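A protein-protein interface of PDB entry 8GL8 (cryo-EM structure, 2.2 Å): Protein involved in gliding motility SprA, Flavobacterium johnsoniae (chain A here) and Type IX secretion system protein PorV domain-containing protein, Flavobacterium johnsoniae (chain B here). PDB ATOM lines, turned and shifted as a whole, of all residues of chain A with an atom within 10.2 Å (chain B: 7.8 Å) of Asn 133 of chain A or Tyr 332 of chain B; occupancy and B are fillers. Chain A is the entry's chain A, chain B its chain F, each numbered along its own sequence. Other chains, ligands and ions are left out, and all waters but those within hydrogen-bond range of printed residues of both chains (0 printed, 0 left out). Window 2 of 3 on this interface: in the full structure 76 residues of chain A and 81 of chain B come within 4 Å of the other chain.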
ATOM      1  N   GLU A 127     -13.820 -11.550 -18.351  1.00  0.00           N
ATOM      2  CA  GLU A 127     -13.716 -11.134 -16.962  1.00  0.00           C
ATOM      3  C   GLU A 127     -12.445 -11.700 -16.346  1.00  0.00           C
ATOM      4  O   GLU A 127     -11.948 -12.751 -16.763  1.00  0.00           O
ATOM      5  CB  GLU A 127     -14.938 -11.587 -16.149  1.00  0.00           C
ATOM      6  CG  GLU A 127     -16.186 -10.752 -16.387  1.00  0.00           C
ATOM      7  CD  GLU A 127     -16.988 -10.523 -15.121  1.00  0.00           C
ATOM      8  OE1 GLU A 127     -17.334 -11.516 -14.446  1.00  0.00           O
ATOM      9  OE2 GLU A 127     -17.277  -9.351 -14.802  1.00  0.00           O
ATOM     10  N   SER A 128     -11.926 -10.993 -15.347  1.00  0.00           N
ATOM     11  CA  SER A 128     -10.722 -11.417 -14.644  1.00  0.00           C
ATOM     12  C   SER A 128     -11.083 -12.491 -13.617  1.00  0.00           C
ATOM     13  O   SER A 128     -12.208 -12.996 -13.581  1.00  0.00           O
ATOM     14  CB  SER A 128     -10.035 -10.214 -14.004  1.00  0.00           C
ATOM     15  OG  SER A 128     -10.986  -9.287 -13.510  1.00  0.00           O
ATOM     16  N   ILE A 129     -10.117 -12.857 -12.768  1.00  0.00           N
ATOM     17  CA  ILE A 129     -10.370 -13.859 -11.736  1.00  0.00           C
ATOM     18  C   ILE A 129     -11.494 -13.399 -10.816  1.00  0.00           C
ATOM     19  O   ILE A 129     -12.353 -14.191 -10.411  1.00  0.00           O
ATOM     20  CB  ILE A 129      -9.075 -14.173 -10.961  1.00  0.00           C
ATOM     21  CG1 ILE A 129      -9.333 -15.219  -9.875  1.00  0.00           C
ATOM     22  CG2 ILE A 129      -8.454 -12.905 -10.383  1.00  0.00           C
ATOM     23  CD1 ILE A 129      -8.232 -16.249  -9.751  1.00  0.00           C
ATOM     24  N   PHE A 130     -11.509 -12.116 -10.479  1.00  0.00           N
ATOM     25  CA  PHE A 130     -12.662 -11.456  -9.894  1.00  0.00           C
ATOM     26  C   PHE A 130     -13.227 -10.472 -10.911  1.00  0.00           C
ATOM     27  O   PHE A 130     -12.524 -10.009 -11.813  1.00  0.00           O
ATOM     28  CB  PHE A 130     -12.292 -10.749  -8.587  1.00  0.00           C
ATOM     29  CG  PHE A 130     -11.503 -11.608  -7.636  1.00  0.00           C
ATOM     30  CD1 PHE A 130     -12.137 -12.563  -6.858  1.00  0.00           C
ATOM     31  CD2 PHE A 130     -10.132 -11.466  -7.525  1.00  0.00           C
ATOM     32  CE1 PHE A 130     -11.417 -13.359  -5.987  1.00  0.00           C
ATOM     33  CE2 PHE A 130      -9.406 -12.259  -6.656  1.00  0.00           C
ATOM     34  CZ  PHE A 130     -10.049 -13.205  -5.886  1.00  0.00           C
ATOM     35  N   GLY A 131     -14.517 -10.167 -10.765  1.00  0.00           N
ATOM     36  CA  GLY A 131     -15.215  -9.418 -11.798  1.00  0.00           C
ATOM     37  C   GLY A 131     -14.635  -8.042 -12.056  1.00  0.00           C
ATOM     38  O   GLY A 131     -14.758  -7.511 -13.162  1.00  0.00           O
ATOM     39  N   SER A 132     -14.001  -7.447 -11.050  1.00  0.00           N
ATOM     40  CA  SER A 132     -13.375  -6.140 -11.192  1.00  0.00           C
ATOM     41  C   SER A 132     -12.110  -6.125 -10.344  1.00  0.00           C
ATOM     42  O   SER A 132     -11.718  -7.136  -9.755  1.00  0.00           O
ATOM     43  CB  SER A 132     -14.353  -5.024 -10.801  1.00  0.00           C
ATOM     44  OG  SER A 132     -14.773  -5.164  -9.456  1.00  0.00           O
ATOM     45  N   ASN A 133     -11.460  -4.964 -10.287  1.00  0.00           N
ATOM     46  CA  ASN A 133     -10.267  -4.776  -9.475  1.00  0.00           C
ATOM     47  C   ASN A 133     -10.550  -3.993  -8.198  1.00  0.00           C
ATOM     48  O   ASN A 133      -9.616  -3.673  -7.456  1.00  0.00           O
ATOM     49  CB  ASN A 133      -9.174  -4.086 -10.297  1.00  0.00           C
ATOM     50  CG  ASN A 133      -9.223  -2.575 -10.184  1.00  0.00           C
ATOM     51  OD1 ASN A 133     -10.155  -1.934 -10.669  1.00  0.00           O
ATOM     52  ND2 ASN A 133      -8.215  -1.998  -9.541  1.00  0.00           N
ATOM     53  N   THR A 134     -11.815  -3.695  -7.918  1.00  0.00           N
ATOM     54  CA  THR A 134     -12.172  -2.898  -6.753  1.00  0.00           C
ATOM     55  C   THR A 134     -12.126  -3.735  -5.482  1.00  0.00           C
ATOM     56  O   THR A 134     -12.519  -4.905  -5.474  1.00  0.00           O
ATOM     57  CB  THR A 134     -13.566  -2.295  -6.926  1.00  0.00           C
ATOM     58  OG1 THR A 134     -14.416  -3.238  -7.590  1.00  0.00           O
ATOM     59  CG2 THR A 134     -13.495  -1.019  -7.748  1.00  0.00           C
ATOM     60  N   ILE A 135     -11.646  -3.122  -4.404  1.00  0.00           N
ATOM     61  CA  ILE A 135     -11.596  -3.744  -3.085  1.00  0.00           C
ATOM     62  C   ILE A 135     -12.530  -2.962  -2.174  1.00  0.00           C
ATOM     63  O   ILE A 135     -12.400  -1.738  -2.043  1.00  0.00           O
ATOM     64  CB  ILE A 135     -10.167  -3.771  -2.523  1.00  0.00           C
ATOM     65  CG1 ILE A 135      -9.203  -4.378  -3.549  1.00  0.00           C
ATOM     66  CG2 ILE A 135     -10.127  -4.530  -1.204  1.00  0.00           C
ATOM     67  CD1 ILE A 135      -9.081  -5.886  -3.471  1.00  0.00           C
ATOM     68  N   ASP A 136     -13.471  -3.663  -1.543  1.00  0.00           N
ATOM     69  CA  ASP A 136     -14.515  -3.017  -0.765  1.00  0.00           C
ATOM     70  C   ASP A 136     -14.700  -3.634   0.618  1.00  0.00           C
ATOM     71  O   ASP A 136     -15.613  -3.226   1.343  1.00  0.00           O
ATOM     72  CB  ASP A 136     -15.845  -3.056  -1.542  1.00  0.00           C
ATOM     73  CG  ASP A 136     -16.930  -2.213  -0.901  1.00  0.00           C
ATOM     74  OD1 ASP A 136     -16.646  -1.053  -0.539  1.00  0.00           O
ATOM     75  OD2 ASP A 136     -18.067  -2.712  -0.759  1.00  0.00           O
ATOM     76  N   VAL A 137     -13.857  -4.585   1.013  1.00  0.00           N
ATOM     77  CA  VAL A 137     -13.988  -5.209   2.326  1.00  0.00           C
ATOM     78  C   VAL A 137     -13.606  -4.175   3.381  1.00  0.00           C
ATOM     79  O   VAL A 137     -12.455  -3.738   3.445  1.00  0.00           O
ATOM     80  CB  VAL A 137     -13.124  -6.468   2.440  1.00  0.00           C
ATOM     81  CG1 VAL A 137     -13.339  -7.137   3.789  1.00  0.00           C
ATOM     82  CG2 VAL A 137     -13.447  -7.424   1.310  1.00  0.00           C
ATOM     83  N   LYS A 182     -16.768  -6.668  -0.529  1.00  0.00           N
ATOM     84  CA  LYS A 182     -16.589  -7.433  -1.749  1.00  0.00           C
ATOM     85  C   LYS A 182     -15.191  -7.210  -2.303  1.00  0.00           C
ATOM     86  O   LYS A 182     -14.598  -6.141  -2.139  1.00  0.00           O
ATOM     87  CB  LYS A 182     -17.625  -7.045  -2.813  1.00  0.00           C
ATOM     88  CG  LYS A 182     -19.026  -7.558  -2.548  1.00  0.00           C
ATOM     89  CD  LYS A 182     -19.617  -8.195  -3.794  1.00  0.00           C
ATOM     90  CE  LYS A 182     -21.107  -7.928  -3.896  1.00  0.00           C
ATOM     91  NZ  LYS A 182     -21.911  -8.997  -3.245  1.00  0.00           N
ATOM     92  N   ILE A 183     -14.674  -8.241  -2.959  1.00  0.00           N
ATOM     93  CA  ILE A 183     -13.449  -8.170  -3.741  1.00  0.00           C
ATOM     94  C   ILE A 183     -13.826  -8.502  -5.176  1.00  0.00           C
ATOM     95  O   ILE A 183     -14.240  -9.634  -5.472  1.00  0.00           O
ATOM     96  CB  ILE A 183     -12.364  -9.120  -3.216  1.00  0.00           C
ATOM     97  CG1 ILE A 183     -11.860  -8.658  -1.849  1.00  0.00           C
ATOM     98  CG2 ILE A 183     -11.210  -9.204  -4.199  1.00  0.00           C
ATOM     99  CD1 ILE A 183     -11.711  -9.779  -0.848  1.00  0.00           C
ATOM    100  N   GLY A 184     -13.717  -7.511  -6.057  1.00  0.00           N
ATOM    101  CA  GLY A 184     -13.947  -7.705  -7.480  1.00  0.00           C
ATOM    102  C   GLY A 184     -15.312  -8.252  -7.832  1.00  0.00           C
ATOM    103  O   GLY A 184     -15.414  -9.145  -8.682  1.00  0.00           O
ATOM    104  N   THR A 185     -16.358  -7.791  -7.136  1.00  0.00           N
ATOM    105  CA  THR A 185     -17.776  -8.088  -7.372  1.00  0.00           C
ATOM    106  C   THR A 185     -18.044  -9.583  -7.539  1.00  0.00           C
ATOM    107  O   THR A 185     -19.110  -9.974  -8.022  1.00  0.00           O
ATOM    108  CB  THR A 185     -18.361  -7.309  -8.571  1.00  0.00           C
ATOM    109  OG1 THR A 185     -19.727  -7.699  -8.758  1.00  0.00           O
ATOM    110  CG2 THR A 185     -17.633  -7.572  -9.879  1.00  0.00           C
ATOM    111  N   ARG A 186     -17.095 -10.424  -7.130  1.00  0.00           N
ATOM    112  CA  ARG A 186     -17.253 -11.869  -7.223  1.00  0.00           C
ATOM    113  C   ARG A 186     -16.978 -12.516  -5.874  1.00  0.00           C
ATOM    114  O   ARG A 186     -17.573 -13.545  -5.540  1.00  0.00           O
ATOM    115  CB  ARG A 186     -16.326 -12.451  -8.291  1.00  0.00           C
ATOM    116  CG  ARG A 186     -16.765 -12.167  -9.713  1.00  0.00           C
ATOM    117  CD  ARG A 186     -17.220 -13.429 -10.408  1.00  0.00           C
ATOM    118  NE  ARG A 186     -17.086 -13.346 -11.857  1.00  0.00           N
ATOM    119  CZ  ARG A 186     -16.060 -13.832 -12.542  1.00  0.00           C
ATOM    120  NH1 ARG A 186     -15.052 -14.439 -11.938  1.00  0.00           N
ATOM    121  NH2 ARG A 186     -16.048 -13.709 -13.865  1.00  0.00           N
ATOM    122  N   LEU A 187     -16.076 -11.924  -5.097  1.00  0.00           N
ATOM    123  CA  LEU A 187     -15.771 -12.407  -3.758  1.00  0.00           C
ATOM    124  C   LEU A 187     -16.568 -11.597  -2.745  1.00  0.00           C
ATOM    125  O   LEU A 187     -16.560 -10.366  -2.789  1.00  0.00           O
ATOM    126  CB  LEU A 187     -14.274 -12.299  -3.469  1.00  0.00           C
ATOM    127  CG  LEU A 187     -13.716 -13.179  -2.349  1.00  0.00           C
ATOM    128  CD1 LEU A 187     -14.311 -14.576  -2.406  1.00  0.00           C
ATOM    129  CD2 LEU A 187     -12.202 -13.235  -2.436  1.00  0.00           C
ATOM    130  N   VAL A 189     -17.269 -11.087   1.429  1.00  0.00           N
ATOM    131  CA  VAL A 189     -16.652 -11.308   2.730  1.00  0.00           C
ATOM    132  C   VAL A 189     -17.614 -10.821   3.801  1.00  0.00           C
ATOM    133  O   VAL A 189     -18.026  -9.651   3.787  1.00  0.00           O
ATOM    134  CB  VAL A 189     -15.302 -10.586   2.851  1.00  0.00           C
ATOM    135  CG1 VAL A 189     -14.626 -10.949   4.161  1.00  0.00           C
ATOM    136  CG2 VAL A 189     -14.418 -10.919   1.665  1.00  0.00           C
ATOM    137  N   TYR A 209     -17.104 -17.104  -3.092  1.00  0.00           N
ATOM    138  CA  TYR A 209     -16.677 -16.837  -4.457  1.00  0.00           C
ATOM    139  C   TYR A 209     -17.746 -17.359  -5.408  1.00  0.00           C
ATOM    140  O   TYR A 209     -17.985 -18.570  -5.476  1.00  0.00           O
ATOM    141  CB  TYR A 209     -15.329 -17.500  -4.736  1.00  0.00           C
ATOM    142  CG  TYR A 209     -14.849 -17.361  -6.160  1.00  0.00           C
ATOM    143  CD1 TYR A 209     -14.612 -16.112  -6.715  1.00  0.00           C
ATOM    144  CD2 TYR A 209     -14.621 -18.481  -6.947  1.00  0.00           C
ATOM    145  CE1 TYR A 209     -14.168 -15.983  -8.014  1.00  0.00           C
ATOM    146  CE2 TYR A 209     -14.175 -18.361  -8.246  1.00  0.00           C
ATOM    147  CZ  TYR A 209     -13.953 -17.110  -8.776  1.00  0.00           C
ATOM    148  OH  TYR A 209     -13.511 -16.986 -10.072  1.00  0.00           O
ATOM    149  N   ASP B 243       1.175  -8.944 -11.975  1.00  0.00           N
ATOM    150  CA  ASP B 243       1.479  -7.775 -11.151  1.00  0.00           C
ATOM    151  C   ASP B 243       0.378  -7.575 -10.110  1.00  0.00           C
ATOM    152  O   ASP B 243       0.520  -6.779  -9.176  1.00  0.00           O
ATOM    153  CB  ASP B 243       1.677  -6.539 -12.047  1.00  0.00           C
ATOM    154  CG  ASP B 243       1.598  -5.226 -11.289  1.00  0.00           C
ATOM    155  OD1 ASP B 243       0.904  -4.307 -11.770  1.00  0.00           O
ATOM    156  OD2 ASP B 243       2.263  -5.096 -10.240  1.00  0.00           O
ATOM    157  N   TYR B 244      -0.702  -8.343 -10.228  1.00  0.00           N
ATOM    158  CA  TYR B 244      -1.789  -8.328  -9.262  1.00  0.00           C
ATOM    159  C   TYR B 244      -1.964  -9.659  -8.550  1.00  0.00           C
ATOM    160  O   TYR B 244      -2.740  -9.731  -7.592  1.00  0.00           O
ATOM    161  CB  TYR B 244      -3.112  -7.945  -9.942  1.00  0.00           C
ATOM    162  CG  TYR B 244      -3.306  -6.460 -10.144  1.00  0.00           C
ATOM    163  CD1 TYR B 244      -2.383  -5.544  -9.661  1.00  0.00           C
ATOM    164  CD2 TYR B 244      -4.422  -5.974 -10.815  1.00  0.00           C
ATOM    165  CE1 TYR B 244      -2.561  -4.186  -9.845  1.00  0.00           C
ATOM    166  CE2 TYR B 244      -4.608  -4.620 -11.003  1.00  0.00           C
ATOM    167  CZ  TYR B 244      -3.676  -3.730 -10.515  1.00  0.00           C
ATOM    168  OH  TYR B 244      -3.859  -2.379 -10.701  1.00  0.00           O
ATOM    169  N   ASN B 245      -1.273 -10.710  -8.986  1.00  0.00           N
ATOM    170  CA  ASN B 245      -1.437 -12.033  -8.402  1.00  0.00           C
ATOM    171  C   ASN B 245      -0.090 -12.537  -7.914  1.00  0.00           C
ATOM    172  O   ASN B 245       0.907 -12.471  -8.641  1.00  0.00           O
ATOM    173  CB  ASN B 245      -2.046 -13.006  -9.416  1.00  0.00           C
ATOM    174  CG  ASN B 245      -3.519 -12.743  -9.658  1.00  0.00           C
ATOM    175  OD1 ASN B 245      -4.351 -12.952  -8.779  1.00  0.00           O
ATOM    176  ND2 ASN B 245      -3.845 -12.272 -10.854  1.00  0.00           N
ATOM    177  N   LYS B 246      -0.058 -13.026  -6.679  1.00  0.00           N
ATOM    178  CA  LYS B 246       1.160 -13.533  -6.072  1.00  0.00           C
ATOM    179  C   LYS B 246       0.871 -14.859  -5.389  1.00  0.00           C
ATOM    180  O   LYS B 246      -0.211 -15.067  -4.841  1.00  0.00           O
ATOM    181  CB  LYS B 246       1.730 -12.537  -5.056  1.00  0.00           C
ATOM    182  CG  LYS B 246       3.222 -12.318  -5.168  1.00  0.00           C
ATOM    183  CD  LYS B 246       3.664 -11.085  -4.396  1.00  0.00           C
ATOM    184  CE  LYS B 246       3.000 -11.013  -3.032  1.00  0.00           C
ATOM    185  NZ  LYS B 246       3.607  -9.958  -2.177  1.00  0.00           N
ATOM    186  N   LEU B 247       1.852 -15.755  -5.425  1.00  0.00           N
ATOM    187  CA  LEU B 247       1.774 -17.034  -4.728  1.00  0.00           C
ATOM    188  C   LEU B 247       3.100 -17.264  -4.020  1.00  0.00           C
ATOM    189  O   LEU B 247       4.113 -17.539  -4.670  1.00  0.00           O
ATOM    190  CB  LEU B 247       1.458 -18.176  -5.692  1.00  0.00           C
ATOM    191  CG  LEU B 247       1.282 -19.552  -5.046  1.00  0.00           C
ATOM    192  CD1 LEU B 247       0.172 -19.519  -4.007  1.00  0.00           C
ATOM    193  CD2 LEU B 247       1.001 -20.610  -6.099  1.00  0.00           C
ATOM    194  N   GLU B 329       0.589 -18.952   0.197  1.00  0.00           N
ATOM    195  CA  GLU B 329      -0.191 -17.737   0.409  1.00  0.00           C
ATOM    196  C   GLU B 329      -0.450 -17.080  -0.941  1.00  0.00           C
ATOM    197  O   GLU B 329       0.489 -16.629  -1.604  1.00  0.00           O
ATOM    198  CB  GLU B 329       0.538 -16.782   1.353  1.00  0.00           C
ATOM    199  CG  GLU B 329      -0.246 -15.531   1.715  1.00  0.00           C
ATOM    200  CD  GLU B 329       0.534 -14.599   2.624  1.00  0.00           C
ATOM    201  OE1 GLU B 329       1.606 -14.117   2.203  1.00  0.00           O
ATOM    202  OE2 GLU B 329       0.079 -14.349   3.759  1.00  0.00           O
ATOM    203  N   TYR B 330      -1.713 -17.035  -1.348  1.00  0.00           N
ATOM    204  CA  TYR B 330      -2.115 -16.314  -2.546  1.00  0.00           C
ATOM    205  C   TYR B 330      -2.497 -14.891  -2.166  1.00  0.00           C
ATOM    206  O   TYR B 330      -3.243 -14.675  -1.208  1.00  0.00           O
ATOM    207  CB  TYR B 330      -3.286 -17.008  -3.241  1.00  0.00           C
ATOM    208  CG  TYR B 330      -3.961 -16.132  -4.269  1.00  0.00           C
ATOM    209  CD1 TYR B 330      -3.355 -15.868  -5.489  1.00  0.00           C
ATOM    210  CD2 TYR B 330      -5.196 -15.556  -4.014  1.00  0.00           C
ATOM    211  CE1 TYR B 330      -3.963 -15.063  -6.428  1.00  0.00           C
ATOM    212  CE2 TYR B 330      -5.811 -14.749  -4.946  1.00  0.00           C
ATOM    213  CZ  TYR B 330      -5.192 -14.505  -6.151  1.00  0.00           C
ATOM    214  OH  TYR B 330      -5.803 -13.702  -7.084  1.00  0.00           O
ATOM    215  N   MET B 331      -1.982 -13.925  -2.916  1.00  0.00           N
ATOM    216  CA  MET B 331      -2.170 -12.515  -2.614  1.00  0.00           C
ATOM    217  C   MET B 331      -2.694 -11.809  -3.855  1.00  0.00           C
ATOM    218  O   MET B 331      -2.098 -11.909  -4.932  1.00  0.00           O
ATOM    219  CB  MET B 331      -0.855 -11.889  -2.136  1.00  0.00           C
ATOM    220  CG  MET B 331      -0.725 -11.826  -0.619  1.00  0.00           C
ATOM    221  SD  MET B 331      -1.513 -10.402   0.151  1.00  0.00           S
ATOM    222  CE  MET B 331      -0.182  -9.210   0.053  1.00  0.00           C
ATOM    223  N   TYR B 332      -3.811 -11.108  -3.699  1.00  0.00           N
ATOM    224  CA  TYR B 332      -4.457 -10.368  -4.773  1.00  0.00           C
ATOM    225  C   TYR B 332      -4.404  -8.882  -4.447  1.00  0.00           C
ATOM    226  O   TYR B 332      -4.923  -8.451  -3.409  1.00  0.00           O
ATOM    227  CB  TYR B 332      -5.903 -10.829  -4.958  1.00  0.00           C
ATOM    228  CG  TYR B 332      -6.654 -10.078  -6.032  1.00  0.00           C
ATOM    229  CD1 TYR B 332      -6.292 -10.191  -7.367  1.00  0.00           C
ATOM    230  CD2 TYR B 332      -7.724  -9.256  -5.712  1.00  0.00           C
ATOM    231  CE1 TYR B 332      -6.975  -9.505  -8.351  1.00  0.00           C
ATOM    232  CE2 TYR B 332      -8.412  -8.567  -6.688  1.00  0.00           C
ATOM    233  CZ  TYR B 332      -8.033  -8.696  -8.006  1.00  0.00           C
ATOM    234  OH  TYR B 332      -8.717  -8.012  -8.984  1.00  0.00           O
ATOM    235  N   GLN B 333      -3.763  -8.115  -5.332  1.00  0.00           N
ATOM    236  CA  GLN B 333      -3.669  -6.657  -5.255  1.00  0.00           C
ATOM    237  C   GLN B 333      -3.072  -6.173  -3.942  1.00  0.00           C
ATOM    238  O   GLN B 333      -3.331  -5.039  -3.526  1.00  0.00           O
ATOM    239  CB  GLN B 333      -5.036  -6.003  -5.476  1.00  0.00           C
ATOM    240  CG  GLN B 333      -5.336  -5.686  -6.925  1.00  0.00           C
ATOM    241  CD  GLN B 333      -6.637  -4.934  -7.090  1.00  0.00           C
ATOM    242  OE1 GLN B 333      -6.781  -3.809  -6.614  1.00  0.00           O
ATOM    243  NE2 GLN B 333      -7.595  -5.557  -7.760  1.00  0.00           N
ATOM    244  N   ASP B 334      -2.280  -7.013  -3.278  1.00  0.00           N
ATOM    245  CA  ASP B 334      -1.720  -6.725  -1.960  1.00  0.00           C
ATOM    246  C   ASP B 334      -2.798  -6.395  -0.931  1.00  0.00           C
ATOM    247  O   ASP B 334      -2.500  -5.837   0.128  1.00  0.00           O
ATOM    248  CB  ASP B 334      -0.688  -5.593  -2.026  1.00  0.00           C
ATOM    249  CG  ASP B 334       0.578  -6.002  -2.750  1.00  0.00           C
ATOM    250  OD1 ASP B 334       1.214  -6.989  -2.325  1.00  0.00           O
ATOM    251  OD2 ASP B 334       0.936  -5.336  -3.744  1.00  0.00           O
ATOM    252  N   ALA B 335      -4.053  -6.744  -1.223  1.00  0.00           N
ATOM    253  CA  ALA B 335      -5.175  -6.422  -0.357  1.00  0.00           C
ATOM    254  C   ALA B 335      -5.976  -7.630   0.097  1.00  0.00           C
ATOM    255  O   ALA B 335      -6.643  -7.546   1.133  1.00  0.00           O
ATOM    256  CB  ALA B 335      -6.127  -5.437  -1.055  1.00  0.00           C
ATOM    257  N   PHE B 336      -5.943  -8.737  -0.638  1.00  0.00           N
ATOM    258  CA  PHE B 336      -6.606  -9.963  -0.216  1.00  0.00           C
ATOM    259  C   PHE B 336      -5.578 -11.081  -0.127  1.00  0.00           C
ATOM    260  O   PHE B 336      -4.745 -11.236  -1.020  1.00  0.00           O
ATOM    261  CB  PHE B 336      -7.733 -10.352  -1.178  1.00  0.00           C
ATOM    262  CG  PHE B 336      -8.338 -11.694  -0.887  1.00  0.00           C
ATOM    263  CD1 PHE B 336      -8.979 -11.931   0.315  1.00  0.00           C
ATOM    264  CD2 PHE B 336      -8.259 -12.719  -1.812  1.00  0.00           C
ATOM    265  CE1 PHE B 336      -9.534 -13.163   0.589  1.00  0.00           C
ATOM    266  CE2 PHE B 336      -8.812 -13.954  -1.545  1.00  0.00           C
ATOM    267  CZ  PHE B 336      -9.450 -14.176  -0.342  1.00  0.00           C
ATOM    268  N   ALA B 337      -5.630 -11.851   0.953  1.00  0.00           N
ATOM    269  CA  ALA B 337      -4.680 -12.929   1.178  1.00  0.00           C
ATOM    270  C   ALA B 337      -5.428 -14.197   1.557  1.00  0.00           C
ATOM    271  O   ALA B 337      -6.348 -14.162   2.375  1.00  0.00           O
ATOM    272  CB  ALA B 337      -3.674 -12.568   2.275  1.00  0.00           C
ATOM    273  N   MET B 338      -5.012 -15.314   0.968  1.00  0.00           N
ATOM    274  CA  MET B 338      -5.633 -16.610   1.200  1.00  0.00           C
ATOM    275  C   MET B 338      -4.515 -17.604   1.472  1.00  0.00           C
ATOM    276  O   MET B 338      -3.660 -17.824   0.610  1.00  0.00           O
ATOM    277  CB  MET B 338      -6.467 -17.031  -0.013  1.00  0.00           C
ATOM    278  CG  MET B 338      -7.149 -18.365   0.125  1.00  0.00           C
ATOM    279  SD  MET B 338      -8.571 -18.199   1.217  1.00  0.00           S
ATOM    280  CE  MET B 338      -8.421 -19.689   2.180  1.00  0.00           C
ATOM    281  N   GLY B 360      -6.763 -12.817   4.886  1.00  0.00           N
ATOM    282  CA  GLY B 360      -6.301 -11.487   5.234  1.00  0.00           C
ATOM    283  C   GLY B 360      -6.870 -10.405   4.341  1.00  0.00           C
ATOM    284  O   GLY B 360      -7.029 -10.610   3.136  1.00  0.00           O
ATOM    285  N   LYS B 362      -7.049  -5.899   3.655  1.00  0.00           N
ATOM    286  CA  LYS B 362      -6.437  -4.593   3.883  1.00  0.00           C
ATOM    287  C   LYS B 362      -7.361  -3.522   3.320  1.00  0.00           C
ATOM    288  O   LYS B 362      -7.550  -3.445   2.103  1.00  0.00           O
ATOM    289  CB  LYS B 362      -5.055  -4.513   3.236  1.00  0.00           C
ATOM    290  CG  LYS B 362      -4.322  -3.210   3.490  1.00  0.00           C
ATOM    291  CD  LYS B 362      -3.482  -2.812   2.291  1.00  0.00           C
ATOM    292  CE  LYS B 362      -2.031  -3.219   2.471  1.00  0.00           C
ATOM    293  NZ  LYS B 362      -1.288  -3.216   1.180  1.00  0.00           N
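The side-chain hydroxyl (OH) of Tyr 332 of chain B is in hydrogen-bond range of the backbone carbonyl oxygen (O) of Ser 132 of chain A, 3.2 Å away. O of Asn 133 of chain A is in hydrogen-bond range of NE2 of Gln 333 of chain B (2.8 Å).
The side-chain hydroxyl of Ser 128 of chain A sits at hydrogen-bond distance from the backbone carbonyl oxygen of Phe 130 of chain A, at 2.4 Å. The side-chain hydroxyl (OG) of Ser 132 of chain A lies within hydrogen-bond range of the side-chain hydroxyl (OG1) of Thr 134 of chain A, 2.7 Å away. N of Ser 132 of chain A is in hydrogen-bond range of O of Gly 184 of chain A, 3.2 Å away. O of Tyr 244 of chain B sits at hydrogen-bond distance from N of Gln 333 of chain B (3.0 Å). The backbone NH (N) of Tyr 330 of chain B sits at hydrogen-bond distance from the backbone carbonyl oxygen (O) of Met 338 of chain B (2.9 Å). The backbone carbonyl oxygen (O) of Ala 335 of chain B is in hydrogen-bond range of the backbone NH (N) of Lys 362 of chain B, at 3.0 Å.
Tyr 330 of chain B touches Phe 130 of chain A. CE2 of Tyr 332 of chain B touches CD2 of Phe 130 of chain A, 3.5 Å away. Tyr 332 of chain B touches Asn 133 of chain A (OH to CA, 3.6 Å). Ile 135 of chain A touches Gln 333 of chain B (CG1 to OE1, 3.9 Å). Ala 335 of chain B touches Ile 135 of chain A (CB to CD1, 3.8 Å). CG2 of Ile 183 of chain A touches CE2 of Tyr 332 of chain B (3.8 Å). Ile 183 of chain A touches Phe 336 of chain B. Phe 336 of chain B touches Leu 187 of chain A.
Of the printed residues of chain B, Asn 133 of chain A touches Tyr 332 and Gln 333. Of chain A, only Phe 130, Ser 132, Asn 133 and Ile 183 come within 4 Å of Tyr 332 of chain B. Of the printed residues of chain B, Ser 132 of chain A touches Tyr 332. No residue of chain A comes within 4 Å of Met 331 of chain B. Of the printed residues of chain B, Ile 135 of chain A touches Gln 333 and Ala 335. Of the printed residues of chain A, Phe 336 of chain B touches Ile 183 and Leu 187. Ser 128 of chain A touches none of the printed residues of chain B. The nearest printed residue of chain B that does not touch Leu 187 of chain A is Tyr 332 of chain B (6.8 Å).
Hydrophobic or aromatic side chains of chain B that line the printed part of chain A: Tyr 330, Tyr 332, Ala 335 and Phe 336. Printed residues of chain A that touch a printed residue of chain B: Phe 130, Ser 132, Asn 133, Ile 135, Ile 183 and Leu 187.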
